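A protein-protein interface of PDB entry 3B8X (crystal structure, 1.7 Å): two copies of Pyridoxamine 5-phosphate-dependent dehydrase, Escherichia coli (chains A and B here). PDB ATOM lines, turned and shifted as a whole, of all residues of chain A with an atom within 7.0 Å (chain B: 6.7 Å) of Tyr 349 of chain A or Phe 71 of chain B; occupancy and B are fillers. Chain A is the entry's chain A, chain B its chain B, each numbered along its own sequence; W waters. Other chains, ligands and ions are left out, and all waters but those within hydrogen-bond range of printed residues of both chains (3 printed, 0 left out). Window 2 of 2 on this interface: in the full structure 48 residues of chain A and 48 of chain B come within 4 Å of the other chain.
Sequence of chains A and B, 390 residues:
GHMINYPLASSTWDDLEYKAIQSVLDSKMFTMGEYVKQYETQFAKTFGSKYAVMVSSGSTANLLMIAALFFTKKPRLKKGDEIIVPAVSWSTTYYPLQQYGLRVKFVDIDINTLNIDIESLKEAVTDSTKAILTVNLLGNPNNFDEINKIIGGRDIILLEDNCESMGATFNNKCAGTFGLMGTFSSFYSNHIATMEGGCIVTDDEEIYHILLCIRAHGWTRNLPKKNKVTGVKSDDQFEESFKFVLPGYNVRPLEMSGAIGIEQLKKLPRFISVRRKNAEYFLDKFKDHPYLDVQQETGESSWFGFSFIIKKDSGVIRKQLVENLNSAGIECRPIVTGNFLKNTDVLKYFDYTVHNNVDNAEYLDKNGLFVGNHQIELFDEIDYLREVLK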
ATOM      1  N   GLN A  98       3.591 -17.224  11.978  1.00  0.00           N
ATOM      2  CA  GLN A  98       2.631 -17.344  10.895  1.00  0.00           C
ATOM      3  C   GLN A  98       2.857 -18.620  10.124  1.00  0.00           C
ATOM      4  O   GLN A  98       1.905 -19.319   9.712  1.00  0.00           O
ATOM      5  CB  GLN A  98       2.754 -16.142   9.970  1.00  0.00           C
ATOM      6  CG  GLN A  98       1.743 -16.043   8.835  1.00  0.00           C
ATOM      7  CD  GLN A  98       2.078 -16.935   7.647  1.00  0.00           C
ATOM      8  OE1 GLN A  98       3.218 -17.369   7.458  1.00  0.00           O
ATOM      9  NE2 GLN A  98       1.065 -17.256   6.869  1.00  0.00           N
ATOM     10  N   GLN A  99       4.127 -18.934   9.935  1.00  0.00           N
ATOM     11  CA  GLN A  99       4.509 -20.114   9.190  1.00  0.00           C
ATOM     12  C   GLN A  99       4.072 -21.402   9.847  1.00  0.00           C
ATOM     13  O   GLN A  99       3.866 -22.408   9.184  1.00  0.00           O
ATOM     14  CB  GLN A  99       6.020 -20.070   8.888  1.00  0.00           C
ATOM     15  CG  GLN A  99       6.274 -19.029   7.795  1.00  0.00           C
ATOM     16  CD  GLN A  99       7.599 -18.274   7.887  1.00  0.00           C
ATOM     17  OE1 GLN A  99       7.949 -17.504   6.964  1.00  0.00           O
ATOM     18  NE2 GLN A  99       8.351 -18.497   8.974  1.00  0.00           N
ATOM     19  N   THR A 344      -0.310  -3.932   7.605  1.00  0.00           N
ATOM     20  CA  THR A 344      -1.611  -4.428   7.217  1.00  0.00           C
ATOM     21  C   THR A 344      -1.530  -5.569   6.225  1.00  0.00           C
ATOM     22  O   THR A 344      -2.275  -6.554   6.312  1.00  0.00           O
ATOM     23  CB  THR A 344      -2.381  -3.287   6.526  1.00  0.00           C
ATOM     24  OG1 THR A 344      -2.248  -2.086   7.294  1.00  0.00           O
ATOM     25  CG2 THR A 344      -3.845  -3.636   6.379  1.00  0.00           C
ATOM     26  N   ASP A 345      -0.664  -5.384   5.241  1.00  0.00           N
ATOM     27  CA  ASP A 345      -0.516  -6.339   4.160  1.00  0.00           C
ATOM     28  C   ASP A 345      -0.014  -7.686   4.633  1.00  0.00           C
ATOM     29  O   ASP A 345      -0.667  -8.713   4.418  1.00  0.00           O
ATOM     30  CB  ASP A 345       0.452  -5.796   3.110  1.00  0.00           C
ATOM     31  CG  ASP A 345      -0.103  -4.602   2.349  1.00  0.00           C
ATOM     32  OD1 ASP A 345      -1.347  -4.431   2.271  1.00  0.00           O
ATOM     33  OD2 ASP A 345       0.732  -3.839   1.811  1.00  0.00           O
ATOM     34  N   VAL A 346       1.182  -7.680   5.216  1.00  0.00           N
ATOM     35  CA  VAL A 346       1.766  -8.919   5.697  1.00  0.00           C
ATOM     36  C   VAL A 346       0.821  -9.523   6.752  1.00  0.00           C
ATOM     37  O   VAL A 346       0.650 -10.725   6.832  1.00  0.00           O
ATOM     38  CB  VAL A 346       3.219  -8.690   6.218  1.00  0.00           C
ATOM     39  CG1 VAL A 346       3.241  -8.358   7.709  1.00  0.00           C
ATOM     40  CG2 VAL A 346       4.116  -9.886   5.955  1.00  0.00           C
ATOM     41  N   LEU A 347       0.124  -8.679   7.507  1.00  0.00           N
ATOM     42  CA  LEU A 347      -0.757  -9.172   8.550  1.00  0.00           C
ATOM     43  C   LEU A 347      -1.940  -9.906   7.997  1.00  0.00           C
ATOM     44  O   LEU A 347      -2.577 -10.675   8.728  1.00  0.00           O
ATOM     45  CB  LEU A 347      -1.196  -8.068   9.504  1.00  0.00           C
ATOM     46  CG  LEU A 347      -0.085  -7.777  10.500  1.00  0.00           C
ATOM     47  CD1 LEU A 347      -0.354  -6.448  11.172  1.00  0.00           C
ATOM     48  CD2 LEU A 347      -0.076  -8.882  11.523  1.00  0.00           C
ATOM     49  N   LYS A 348      -2.185  -9.695   6.704  1.00  0.00           N
ATOM     50  CA  LYS A 348      -3.244 -10.378   5.968  1.00  0.00           C
ATOM     51  C   LYS A 348      -2.997 -11.892   5.995  1.00  0.00           C
ATOM     52  O   LYS A 348      -3.909 -12.701   5.815  1.00  0.00           O
ATOM     53  CB  LYS A 348      -3.176  -9.924   4.512  1.00  0.00           C
ATOM     54  CG  LYS A 348      -4.381  -9.157   4.043  1.00  0.00           C
ATOM     55  CD  LYS A 348      -4.105  -8.530   2.694  1.00  0.00           C
ATOM     56  CE  LYS A 348      -4.838  -7.209   2.537  1.00  0.00           C
ATOM     57  NZ  LYS A 348      -4.740  -6.723   1.130  1.00  0.00           N
ATOM     58  N   TYR A 349      -1.742 -12.286   6.167  1.00  0.00           N
ATOM     59  CA  TYR A 349      -1.383 -13.706   6.165  1.00  0.00           C
ATOM     60  C   TYR A 349      -1.472 -14.320   7.553  1.00  0.00           C
ATOM     61  O   TYR A 349      -1.470 -15.541   7.707  1.00  0.00           O
ATOM     62  CB  TYR A 349       0.013 -13.930   5.557  1.00  0.00           C
ATOM     63  CG  TYR A 349       0.176 -13.472   4.115  1.00  0.00           C
ATOM     64  CD1 TYR A 349       0.645 -12.191   3.799  1.00  0.00           C
ATOM     65  CD2 TYR A 349      -0.151 -14.317   3.059  1.00  0.00           C
ATOM     66  CE1 TYR A 349       0.802 -11.790   2.483  1.00  0.00           C
ATOM     67  CE2 TYR A 349      -0.056 -13.896   1.732  1.00  0.00           C
ATOM     68  CZ  TYR A 349       0.415 -12.651   1.450  1.00  0.00           C
ATOM     69  OH  TYR A 349       0.575 -12.308   0.139  1.00  0.00           O
ATOM     70  N   PHE A 350      -1.583 -13.485   8.570  1.00  0.00           N
ATOM     71  CA  PHE A 350      -1.643 -13.985   9.920  1.00  0.00           C
ATOM     72  C   PHE A 350      -3.010 -14.259  10.499  1.00  0.00           C
ATOM     73  O   PHE A 350      -3.997 -13.603  10.176  1.00  0.00           O
ATOM     74  CB  PHE A 350      -1.051 -12.944  10.881  1.00  0.00           C
ATOM     75  CG  PHE A 350       0.451 -12.886  10.894  1.00  0.00           C
ATOM     76  CD1 PHE A 350       1.144 -12.431   9.764  1.00  0.00           C
ATOM     77  CD2 PHE A 350       1.168 -13.154  12.057  1.00  0.00           C
ATOM     78  CE1 PHE A 350       2.519 -12.320   9.750  1.00  0.00           C
ATOM     79  CE2 PHE A 350       2.559 -12.961  12.075  1.00  0.00           C
ATOM     80  CZ  PHE A 350       3.232 -12.582  10.907  1.00  0.00           C
ATOM     81  N   ASP A 351      -3.015 -15.149  11.479  1.00  0.00           N
ATOM     82  CA  ASP A 351      -4.191 -15.417  12.282  1.00  0.00           C
ATOM     83  C   ASP A 351      -3.858 -14.614  13.539  1.00  0.00           C
ATOM     84  O   ASP A 351      -3.063 -15.030  14.393  1.00  0.00           O
ATOM     85  CB  ASP A 351      -4.277 -16.913  12.601  1.00  0.00           C
ATOM     86  CG  ASP A 351      -5.365 -17.250  13.630  1.00  0.00           C
ATOM     87  OD1 ASP A 351      -6.282 -16.428  13.831  1.00  0.00           O
ATOM     88  OD2 ASP A 351      -5.315 -18.359  14.202  1.00  0.00           O
ATOM     89  N   TYR A 352      -4.388 -13.403  13.649  1.00  0.00           N
ATOM     90  CA  TYR A 352      -3.973 -12.677  14.833  1.00  0.00           C
ATOM     91  C   TYR A 352      -5.037 -11.843  15.485  1.00  0.00           C
ATOM     92  O   TYR A 352      -6.141 -11.711  14.960  1.00  0.00           O
ATOM     93  CB  TYR A 352      -2.756 -11.796  14.501  1.00  0.00           C
ATOM     94  CG  TYR A 352      -3.176 -10.550  13.744  1.00  0.00           C
ATOM     95  CD1 TYR A 352      -3.204  -9.312  14.353  1.00  0.00           C
ATOM     96  CD2 TYR A 352      -3.553 -10.639  12.408  1.00  0.00           C
ATOM     97  CE1 TYR A 352      -3.659  -8.206  13.650  1.00  0.00           C
ATOM     98  CE2 TYR A 352      -3.958  -9.555  11.697  1.00  0.00           C
ATOM     99  CZ  TYR A 352      -4.030  -8.344  12.324  1.00  0.00           C
ATOM    100  OH  TYR A 352      -4.419  -7.267  11.565  1.00  0.00           O
ATOM    101  N   LEU B  64      12.040 -21.465  -0.569  1.00  0.00           N
ATOM    102  CA  LEU B  64      11.581 -20.237  -1.248  1.00  0.00           C
ATOM    103  C   LEU B  64      10.795 -20.517  -2.512  1.00  0.00           C
ATOM    104  O   LEU B  64       9.914 -19.716  -2.861  1.00  0.00           O
ATOM    105  CB  LEU B  64      12.748 -19.282  -1.550  1.00  0.00           C
ATOM    106  CG  LEU B  64      13.505 -18.636  -0.357  1.00  0.00           C
ATOM    107  CD1 LEU B  64      14.192 -17.310  -0.640  1.00  0.00           C
ATOM    108  CD2 LEU B  64      12.657 -18.483   0.870  1.00  0.00           C
ATOM    109  N   ILE B  66       8.689 -22.941  -3.188  1.00  0.00           N
ATOM    110  CA  ILE B  66       7.291 -23.203  -2.769  1.00  0.00           C
ATOM    111  C   ILE B  66       6.606 -21.969  -2.160  1.00  0.00           C
ATOM    112  O   ILE B  66       5.470 -21.612  -2.458  1.00  0.00           O
ATOM    113  CB  ILE B  66       7.250 -24.376  -1.731  1.00  0.00           C
ATOM    114  CG1 ILE B  66       7.877 -25.610  -2.356  1.00  0.00           C
ATOM    115  CG2 ILE B  66       5.831 -24.653  -1.277  1.00  0.00           C
ATOM    116  CD1 ILE B  66       7.267 -25.944  -3.728  1.00  0.00           C
ATOM    117  N   ALA B  67       7.286 -21.324  -1.237  1.00  0.00           N
ATOM    118  CA  ALA B  67       6.697 -20.165  -0.592  1.00  0.00           C
ATOM    119  C   ALA B  67       6.281 -19.070  -1.562  1.00  0.00           C
ATOM    120  O   ALA B  67       5.217 -18.447  -1.444  1.00  0.00           O
ATOM    121  CB  ALA B  67       7.679 -19.623   0.389  1.00  0.00           C
ATOM    122  N   ALA B  68       7.166 -18.744  -2.487  1.00  0.00           N
ATOM    123  CA  ALA B  68       6.831 -17.680  -3.414  1.00  0.00           C
ATOM    124  C   ALA B  68       5.481 -17.850  -4.103  1.00  0.00           C
ATOM    125  O   ALA B  68       4.836 -16.868  -4.399  1.00  0.00           O
ATOM    126  CB  ALA B  68       7.918 -17.540  -4.436  1.00  0.00           C
ATOM    127  N   LEU B  69       5.088 -19.086  -4.398  1.00  0.00           N
ATOM    128  CA  LEU B  69       3.841 -19.350  -5.089  1.00  0.00           C
ATOM    129  C   LEU B  69       2.597 -18.955  -4.305  1.00  0.00           C
ATOM    130  O   LEU B  69       1.507 -18.856  -4.851  1.00  0.00           O
ATOM    131  CB  LEU B  69       3.753 -20.815  -5.505  1.00  0.00           C
ATOM    132  CG  LEU B  69       4.864 -21.243  -6.459  1.00  0.00           C
ATOM    133  CD1 LEU B  69       4.967 -22.768  -6.612  1.00  0.00           C
ATOM    134  CD2 LEU B  69       4.720 -20.536  -7.785  1.00  0.00           C
ATOM    135  N   PHE B  70       2.777 -18.684  -3.023  1.00  0.00           N
ATOM    136  CA  PHE B  70       1.661 -18.307  -2.177  1.00  0.00           C
ATOM    137  C   PHE B  70       1.529 -16.801  -2.156  1.00  0.00           C
ATOM    138  O   PHE B  70       0.543 -16.256  -1.670  1.00  0.00           O
ATOM    139  CB  PHE B  70       1.879 -18.833  -0.752  1.00  0.00           C
ATOM    140  CG  PHE B  70       1.682 -20.317  -0.616  1.00  0.00           C
ATOM    141  CD1 PHE B  70       2.587 -21.207  -1.198  1.00  0.00           C
ATOM    142  CD2 PHE B  70       0.590 -20.826   0.106  1.00  0.00           C
ATOM    143  CE1 PHE B  70       2.371 -22.568  -1.132  1.00  0.00           C
ATOM    144  CE2 PHE B  70       0.339 -22.189   0.155  1.00  0.00           C
ATOM    145  CZ  PHE B  70       1.258 -23.075  -0.415  1.00  0.00           C
ATOM    146  N   PHE B  71       2.562 -16.141  -2.657  1.00  0.00           N
ATOM    147  CA  PHE B  71       2.731 -14.698  -2.532  1.00  0.00           C
ATOM    148  C   PHE B  71       2.550 -13.936  -3.809  1.00  0.00           C
ATOM    149  O   PHE B  71       2.668 -12.717  -3.830  1.00  0.00           O
ATOM    150  CB  PHE B  71       4.071 -14.339  -1.829  1.00  0.00           C
ATOM    151  CG  PHE B  71       4.248 -15.015  -0.492  1.00  0.00           C
ATOM    152  CD1 PHE B  71       5.403 -15.697  -0.184  1.00  0.00           C
ATOM    153  CD2 PHE B  71       3.229 -15.015   0.446  1.00  0.00           C
ATOM    154  CE1 PHE B  71       5.521 -16.334   1.040  1.00  0.00           C
ATOM    155  CE2 PHE B  71       3.329 -15.684   1.650  1.00  0.00           C
ATOM    156  CZ  PHE B  71       4.479 -16.344   1.954  1.00  0.00           C
ATOM    157  N   THR B  72       2.194 -14.623  -4.883  1.00  0.00           N
ATOM    158  CA  THR B  72       2.028 -13.845  -6.098  1.00  0.00           C
ATOM    159  C   THR B  72       0.697 -13.094  -5.943  1.00  0.00           C
ATOM    160  O   THR B  72      -0.176 -13.523  -5.188  1.00  0.00           O
ATOM    161  CB  THR B  72       1.987 -14.778  -7.275  1.00  0.00           C
ATOM    162  OG1 THR B  72       1.251 -15.944  -6.876  1.00  0.00           O
ATOM    163  CG2 THR B  72       3.441 -15.173  -7.654  1.00  0.00           C
ATOM    164  N   LYS B  73       0.568 -11.954  -6.617  1.00  0.00           N
ATOM    165  CA  LYS B  73      -0.646 -11.110  -6.573  1.00  0.00           C
ATOM    166  C   LYS B  73      -1.960 -11.896  -6.751  1.00  0.00           C
ATOM    167  O   LYS B  73      -2.902 -11.735  -5.965  1.00  0.00           O
ATOM    168  CB  LYS B  73      -0.512  -9.951  -7.547  1.00  0.00           C
ATOM    169  CG  LYS B  73       0.694  -9.038  -7.276  1.00  0.00           C
ATOM    170  CD  LYS B  73       0.546  -8.383  -5.905  1.00  0.00           C
ATOM    171  CE  LYS B  73       1.809  -7.675  -5.442  1.00  0.00           C
ATOM    172  NZ  LYS B  73       1.514  -6.875  -4.213  1.00  0.00           N
ATOM    173  N   LYS B  74      -1.986 -12.798  -7.739  1.00  0.00           N
ATOM    174  CA  LYS B  74      -3.018 -13.816  -7.893  1.00  0.00           C
ATOM    175  C   LYS B  74      -2.236 -15.028  -7.321  1.00  0.00           C
ATOM    176  O   LYS B  74      -1.297 -15.490  -7.971  1.00  0.00           O
ATOM    177  CB  LYS B  74      -3.290 -14.052  -9.388  1.00  0.00           C
ATOM    178  CG  LYS B  74      -4.371 -15.071  -9.673  1.00  0.00           C
ATOM    179  CD  LYS B  74      -4.894 -14.919 -11.096  1.00  0.00           C
ATOM    180  CE  LYS B  74      -6.315 -15.467 -11.242  1.00  0.00           C
ATOM    181  NZ  LYS B  74      -7.299 -14.854 -10.295  1.00  0.00           N
ATOM    182  N   PRO B  75      -2.528 -15.492  -6.109  1.00  0.00           N
ATOM    183  CA  PRO B  75      -1.745 -16.595  -5.527  1.00  0.00           C
ATOM    184  C   PRO B  75      -1.764 -17.835  -6.379  1.00  0.00           C
ATOM    185  O   PRO B  75      -2.817 -18.353  -6.711  1.00  0.00           O
ATOM    186  CB  PRO B  75      -2.486 -16.912  -4.238  1.00  0.00           C
ATOM    187  CG  PRO B  75      -3.152 -15.616  -3.871  1.00  0.00           C
ATOM    188  CD  PRO B  75      -3.557 -14.993  -5.178  1.00  0.00           C
ATOM    189  N   ARG B  76      -0.595 -18.351  -6.707  1.00  0.00           N
ATOM    190  CA  ARG B  76      -0.552 -19.535  -7.542  1.00  0.00           C
ATOM    191  C   ARG B  76      -0.810 -20.863  -6.857  1.00  0.00           C
ATOM    192  O   ARG B  76      -1.078 -21.844  -7.546  1.00  0.00           O
ATOM    193  CB  ARG B  76       0.701 -19.550  -8.377  1.00  0.00           C
ATOM    194  CG  ARG B  76       0.607 -18.652  -9.592  1.00  0.00           C
ATOM    195  CD  ARG B  76       1.782 -17.719  -9.685  1.00  0.00           C
ATOM    196  NE  ARG B  76       2.288 -17.718 -11.055  1.00  0.00           N
ATOM    197  CZ  ARG B  76       2.924 -16.708 -11.647  1.00  0.00           C
ATOM    198  NH1 ARG B  76       3.188 -15.568 -11.003  1.00  0.00           N
ATOM    199  NH2 ARG B  76       3.318 -16.854 -12.905  1.00  0.00           N
ATOM    200  N   LEU B  77      -0.762 -20.889  -5.522  1.00  0.00           N
ATOM    201  CA  LEU B  77      -1.076 -22.086  -4.728  1.00  0.00           C
ATOM    202  C   LEU B  77      -1.695 -21.579  -3.455  1.00  0.00           C
ATOM    203  O   LEU B  77      -1.471 -20.416  -3.096  1.00  0.00           O
ATOM    204  CB  LEU B  77       0.166 -22.949  -4.368  1.00  0.00           C
ATOM    205  CG  LEU B  77       0.931 -23.737  -5.456  1.00  0.00           C
ATOM    206  CD1 LEU B  77       2.150 -24.447  -4.843  1.00  0.00           C
ATOM    207  CD2 LEU B  77       0.055 -24.769  -6.162  1.00  0.00           C
ATOM    208  N   TYR B 100       4.028 -25.710   3.771  1.00  0.00           N
ATOM    209  CA  TYR B 100       3.047 -24.787   3.196  1.00  0.00           C
ATOM    210  C   TYR B 100       1.655 -25.372   3.079  1.00  0.00           C
ATOM    211  O   TYR B 100       0.815 -24.830   2.374  1.00  0.00           O
ATOM    212  CB  TYR B 100       3.523 -24.182   1.888  1.00  0.00           C
ATOM    213  CG  TYR B 100       4.538 -23.103   2.209  1.00  0.00           C
ATOM    214  CD1 TYR B 100       5.832 -23.438   2.636  1.00  0.00           C
ATOM    215  CD2 TYR B 100       4.153 -21.759   2.235  1.00  0.00           C
ATOM    216  CE1 TYR B 100       6.729 -22.451   3.046  1.00  0.00           C
ATOM    217  CE2 TYR B 100       5.020 -20.792   2.677  1.00  0.00           C
ATOM    218  CZ  TYR B 100       6.295 -21.135   3.084  1.00  0.00           C
ATOM    219  OH  TYR B 100       7.148 -20.109   3.413  1.00  0.00           O
ATOM    220  N   GLU B 206       7.937 -11.348 -11.548  1.00  0.00           N
ATOM    221  CA  GLU B 206       7.200 -11.257 -10.261  1.00  0.00           C
ATOM    222  C   GLU B 206       7.764 -12.231  -9.226  1.00  0.00           C
ATOM    223  O   GLU B 206       7.993 -11.876  -8.057  1.00  0.00           O
ATOM    224  CB  GLU B 206       5.687 -11.504 -10.360  1.00  0.00           C
ATOM    225  CG  GLU B 206       4.953 -11.199  -9.025  1.00  0.00           C
ATOM    226  CD  GLU B 206       3.500 -11.664  -9.015  1.00  0.00           C
ATOM    227  OE1 GLU B 206       3.170 -12.460  -9.912  1.00  0.00           O
ATOM    228  OE2 GLU B 206       2.720 -11.309  -8.093  1.00  0.00           O
ATOM    229  N   ILE B 210       9.555 -11.553  -5.778  1.00  0.00           N
ATOM    230  CA  ILE B 210       9.042 -12.164  -4.549  1.00  0.00           C
ATOM    231  C   ILE B 210      10.190 -12.877  -3.862  1.00  0.00           C
ATOM    232  O   ILE B 210      10.327 -12.857  -2.638  1.00  0.00           O
ATOM    233  CB  ILE B 210       7.932 -13.199  -4.811  1.00  0.00           C
ATOM    234  CG1 ILE B 210       6.593 -12.512  -5.169  1.00  0.00           C
ATOM    235  CG2 ILE B 210       7.718 -14.022  -3.571  1.00  0.00           C
ATOM    236  CD1 ILE B 210       5.539 -13.404  -5.936  1.00  0.00           C
ATOM    237  N   ILE B 214      11.503 -12.325   0.072  1.00  0.00           N
ATOM    238  CA  ILE B 214      11.442 -13.359   1.095  1.00  0.00           C
ATOM    239  C   ILE B 214      12.781 -13.980   1.494  1.00  0.00           C
ATOM    240  O   ILE B 214      12.879 -14.672   2.538  1.00  0.00           O
ATOM    241  CB  ILE B 214      10.372 -14.379   0.810  1.00  0.00           C
ATOM    242  CG1 ILE B 214      10.668 -15.087  -0.523  1.00  0.00           C
ATOM    243  CG2 ILE B 214       9.010 -13.737   0.919  1.00  0.00           C
ATOM    244  CD1 ILE B 214       9.725 -16.288  -0.737  1.00  0.00           C
ATOM    245  N   VAL B 229       6.351  -6.324  -6.131  1.00  0.00           N
ATOM    246  CA  VAL B 229       5.809  -6.681  -4.832  1.00  0.00           C
ATOM    247  C   VAL B 229       5.102  -5.514  -4.215  1.00  0.00           C
ATOM    248  O   VAL B 229       4.017  -5.656  -3.656  1.00  0.00           O
ATOM    249  CB  VAL B 229       6.909  -7.202  -3.793  1.00  0.00           C
ATOM    250  CG1 VAL B 229       6.237  -7.579  -2.482  1.00  0.00           C
ATOM    251  CG2 VAL B 229       7.675  -8.427  -4.384  1.00  0.00           C
ATOM    252  N   VAL B 245       6.913  -6.624   4.174  1.00  0.00           N
ATOM    253  CA  VAL B 245       5.769  -6.898   3.282  1.00  0.00           C
ATOM    254  C   VAL B 245       5.314  -8.290   2.881  1.00  0.00           C
ATOM    255  O   VAL B 245       4.201  -8.439   2.359  1.00  0.00           O
ATOM    256  CB  VAL B 245       5.884  -6.029   1.988  1.00  0.00           C
ATOM    257  CG1 VAL B 245       6.059  -4.561   2.392  1.00  0.00           C
ATOM    258  CG2 VAL B 245       7.112  -6.439   1.124  1.00  0.00           C
ATOM    259  N   LEU B 246       6.165  -9.298   3.053  1.00  0.00           N
ATOM    260  CA  LEU B 246       5.802 -10.690   2.777  1.00  0.00           C
ATOM    261  C   LEU B 246       6.379 -11.503   3.949  1.00  0.00           C
ATOM    262  O   LEU B 246       7.452 -11.137   4.467  1.00  0.00           O
ATOM    263  CB  LEU B 246       6.434 -11.155   1.457  1.00  0.00           C
ATOM    264  CG  LEU B 246       5.671 -10.622   0.252  1.00  0.00           C
ATOM    265  CD1 LEU B 246       6.376 -11.111  -0.959  1.00  0.00           C
ATOM    266  CD2 LEU B 246       4.192 -11.048   0.225  1.00  0.00           C
ATOM    267  N   PRO B 247       5.686 -12.562   4.379  1.00  0.00           N
ATOM    268  CA  PRO B 247       6.204 -13.426   5.453  1.00  0.00           C
ATOM    269  C   PRO B 247       7.373 -14.256   4.895  1.00  0.00           C
ATOM    270  O   PRO B 247       7.177 -15.330   4.351  1.00  0.00           O
ATOM    271  CB  PRO B 247       4.996 -14.316   5.845  1.00  0.00           C
ATOM    272  CG  PRO B 247       3.842 -13.923   4.906  1.00  0.00           C
ATOM    273  CD  PRO B 247       4.435 -13.077   3.787  1.00  0.00           C
ATOM    274  N   GLY B 248       8.598 -13.762   5.057  1.00  0.00           N
ATOM    275  CA  GLY B 248       9.779 -14.455   4.539  1.00  0.00           C
ATOM    276  C   GLY B 248      10.759 -15.034   5.591  1.00  0.00           C
ATOM    277  O   GLY B 248      10.396 -15.368   6.749  1.00  0.00           O
ATOM    278  N   TYR B 249      12.019 -15.100   5.186  1.00  0.00           N
ATOM    279  CA  TYR B 249      13.039 -15.694   6.059  1.00  0.00           C
ATOM    280  C   TYR B 249      14.278 -14.868   5.905  1.00  0.00           C
ATOM    281  O   TYR B 249      14.325 -13.922   5.138  1.00  0.00           O
ATOM    282  CB  TYR B 249      13.406 -17.094   5.463  1.00  0.00           C
ATOM    283  CG  TYR B 249      12.227 -18.063   5.430  1.00  0.00           C
ATOM    284  CD1 TYR B 249      11.377 -18.143   4.306  1.00  0.00           C
ATOM    285  CD2 TYR B 249      11.920 -18.849   6.551  1.00  0.00           C
ATOM    286  CE1 TYR B 249      10.231 -18.984   4.333  1.00  0.00           C
ATOM    287  CE2 TYR B 249      10.751 -19.672   6.597  1.00  0.00           C
ATOM    288  CZ  TYR B 249       9.920 -19.764   5.464  1.00  0.00           C
ATOM    289  OH  TYR B 249       8.800 -20.613   5.465  1.00  0.00           O
HETATM  290  O   HOH W   1       6.185 -17.792   4.456  1.00  0.00           O
HETATM  291  O   HOH W   2      10.587 -16.704   9.050  1.00  0.00           O
HETATM  292  O   HOH W   3      -0.760 -13.705  -2.060  1.00  0.00           O
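The side-chain amide oxygen (OE1) of Gln 99 of chain A lies close to the backbone carbonyl oxygen (O) of Pro 247 of chain B. OE1 of Gln 99 of chain A lies close to O of Gly 248 of chain B (3.3 Å).
O of Tyr 349 of chain A is in hydrogen-bond range of NE2 of Gln 98 of chain A, at 3.2 Å. OH of Tyr 249 of chain B is in hydrogen-bond range of OH of Tyr 100 of chain B, at 2.7 Å. The backbone NH (N) of Tyr 249 of chain B is in hydrogen-bond range of the backbone carbonyl oxygen (O) of Ile 214 of chain B, 2.8 Å away.
OE1 of Gln 98 of chain A touches CB of Pro 247 of chain B, 3.9 Å away. Tyr 249 of chain B touches Gln 99 of chain A. Val 346 of chain A touches Val 245 of chain B. Val 346 of chain A touches Leu 246 of chain B. N of Pro 247 of chain B touches CG2 of Val 346 of chain A (3.5 Å). Tyr 349 of chain A touches Phe 71 of chain B. OH of Tyr 349 of chain A touches CD2 of Leu 246 of chain B (3.8 Å). CG of Pro 247 of chain B touches CG of Tyr 349 of chain A, 3.8 Å away.
Lys 348 of chain A touches none of the printed residues of chain B. Ile 66 of chain B touches none of the printed residues of chain A. Phe 71 of chain B touches just one residue of chain A: Tyr 349 (3.7 Å). Of the printed residues of chain A, Gly 248 of chain B touches Gln 99 (3.3 Å). Printed residues of chain A within 4 Å of Tyr 249 of chain B: Gln 99 (3.4 Å). The nearest residue of chain B that does not touch Tyr 349 of chain A is Phe 70 of chain B (4.2 Å). The nearest printed residue of chain A that does not touch Leu 246 of chain B is Asp 345 of chain A (6.6 Å).
Of the 11 printed residues of chain A, 4 touch a printed residue of chain B. Hydrophobic or aromatic side chains of chain A that line the printed part of chain B: Val 346 and Tyr 349. Of the 23 printed residues of chain B, 6 touch a printed residue of chain A. Hydrophobic or aromatic side chains of chain B within 4 Å of the printed part of chain A: Phe 71, Leu 246, Pro 247 and Tyr 249. Among the printed residues, 10 pairs touch across the chains. Among the printed residues, no Asp or Glu carboxylate lies within 4 Å of a Lys or Arg side-chain nitrogen of the other chain.
No position is printed for both chains. Of the 10 pairs that touch across the chains among the printed residues, none has its exchanged pair printed and touching as well.
Water W1 lies within hydrogen-bond range of the backbone carbonyl oxygen (O) of Pro 247 of chain B, the side-chain hydroxyl (OH) of Tyr 100 of chain B and the side-chain amide oxygen (OE1) of Gln 99 of chain A. Water W2 lies within hydrogen-bond range of the backbone carbonyl oxygen (O) of Gly 248 of chain B and the side-chain amide nitrogen (NE2) of Gln 99 of chain A. Water W3 lies within hydrogen-bond range of the backbone carbonyl oxygen (O) of Phe 70 of chain B, the side-chain hydroxyl (OH) of Tyr 349 of chain A and the backbone carbonyl oxygen (O) of Thr 72 of chain B.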
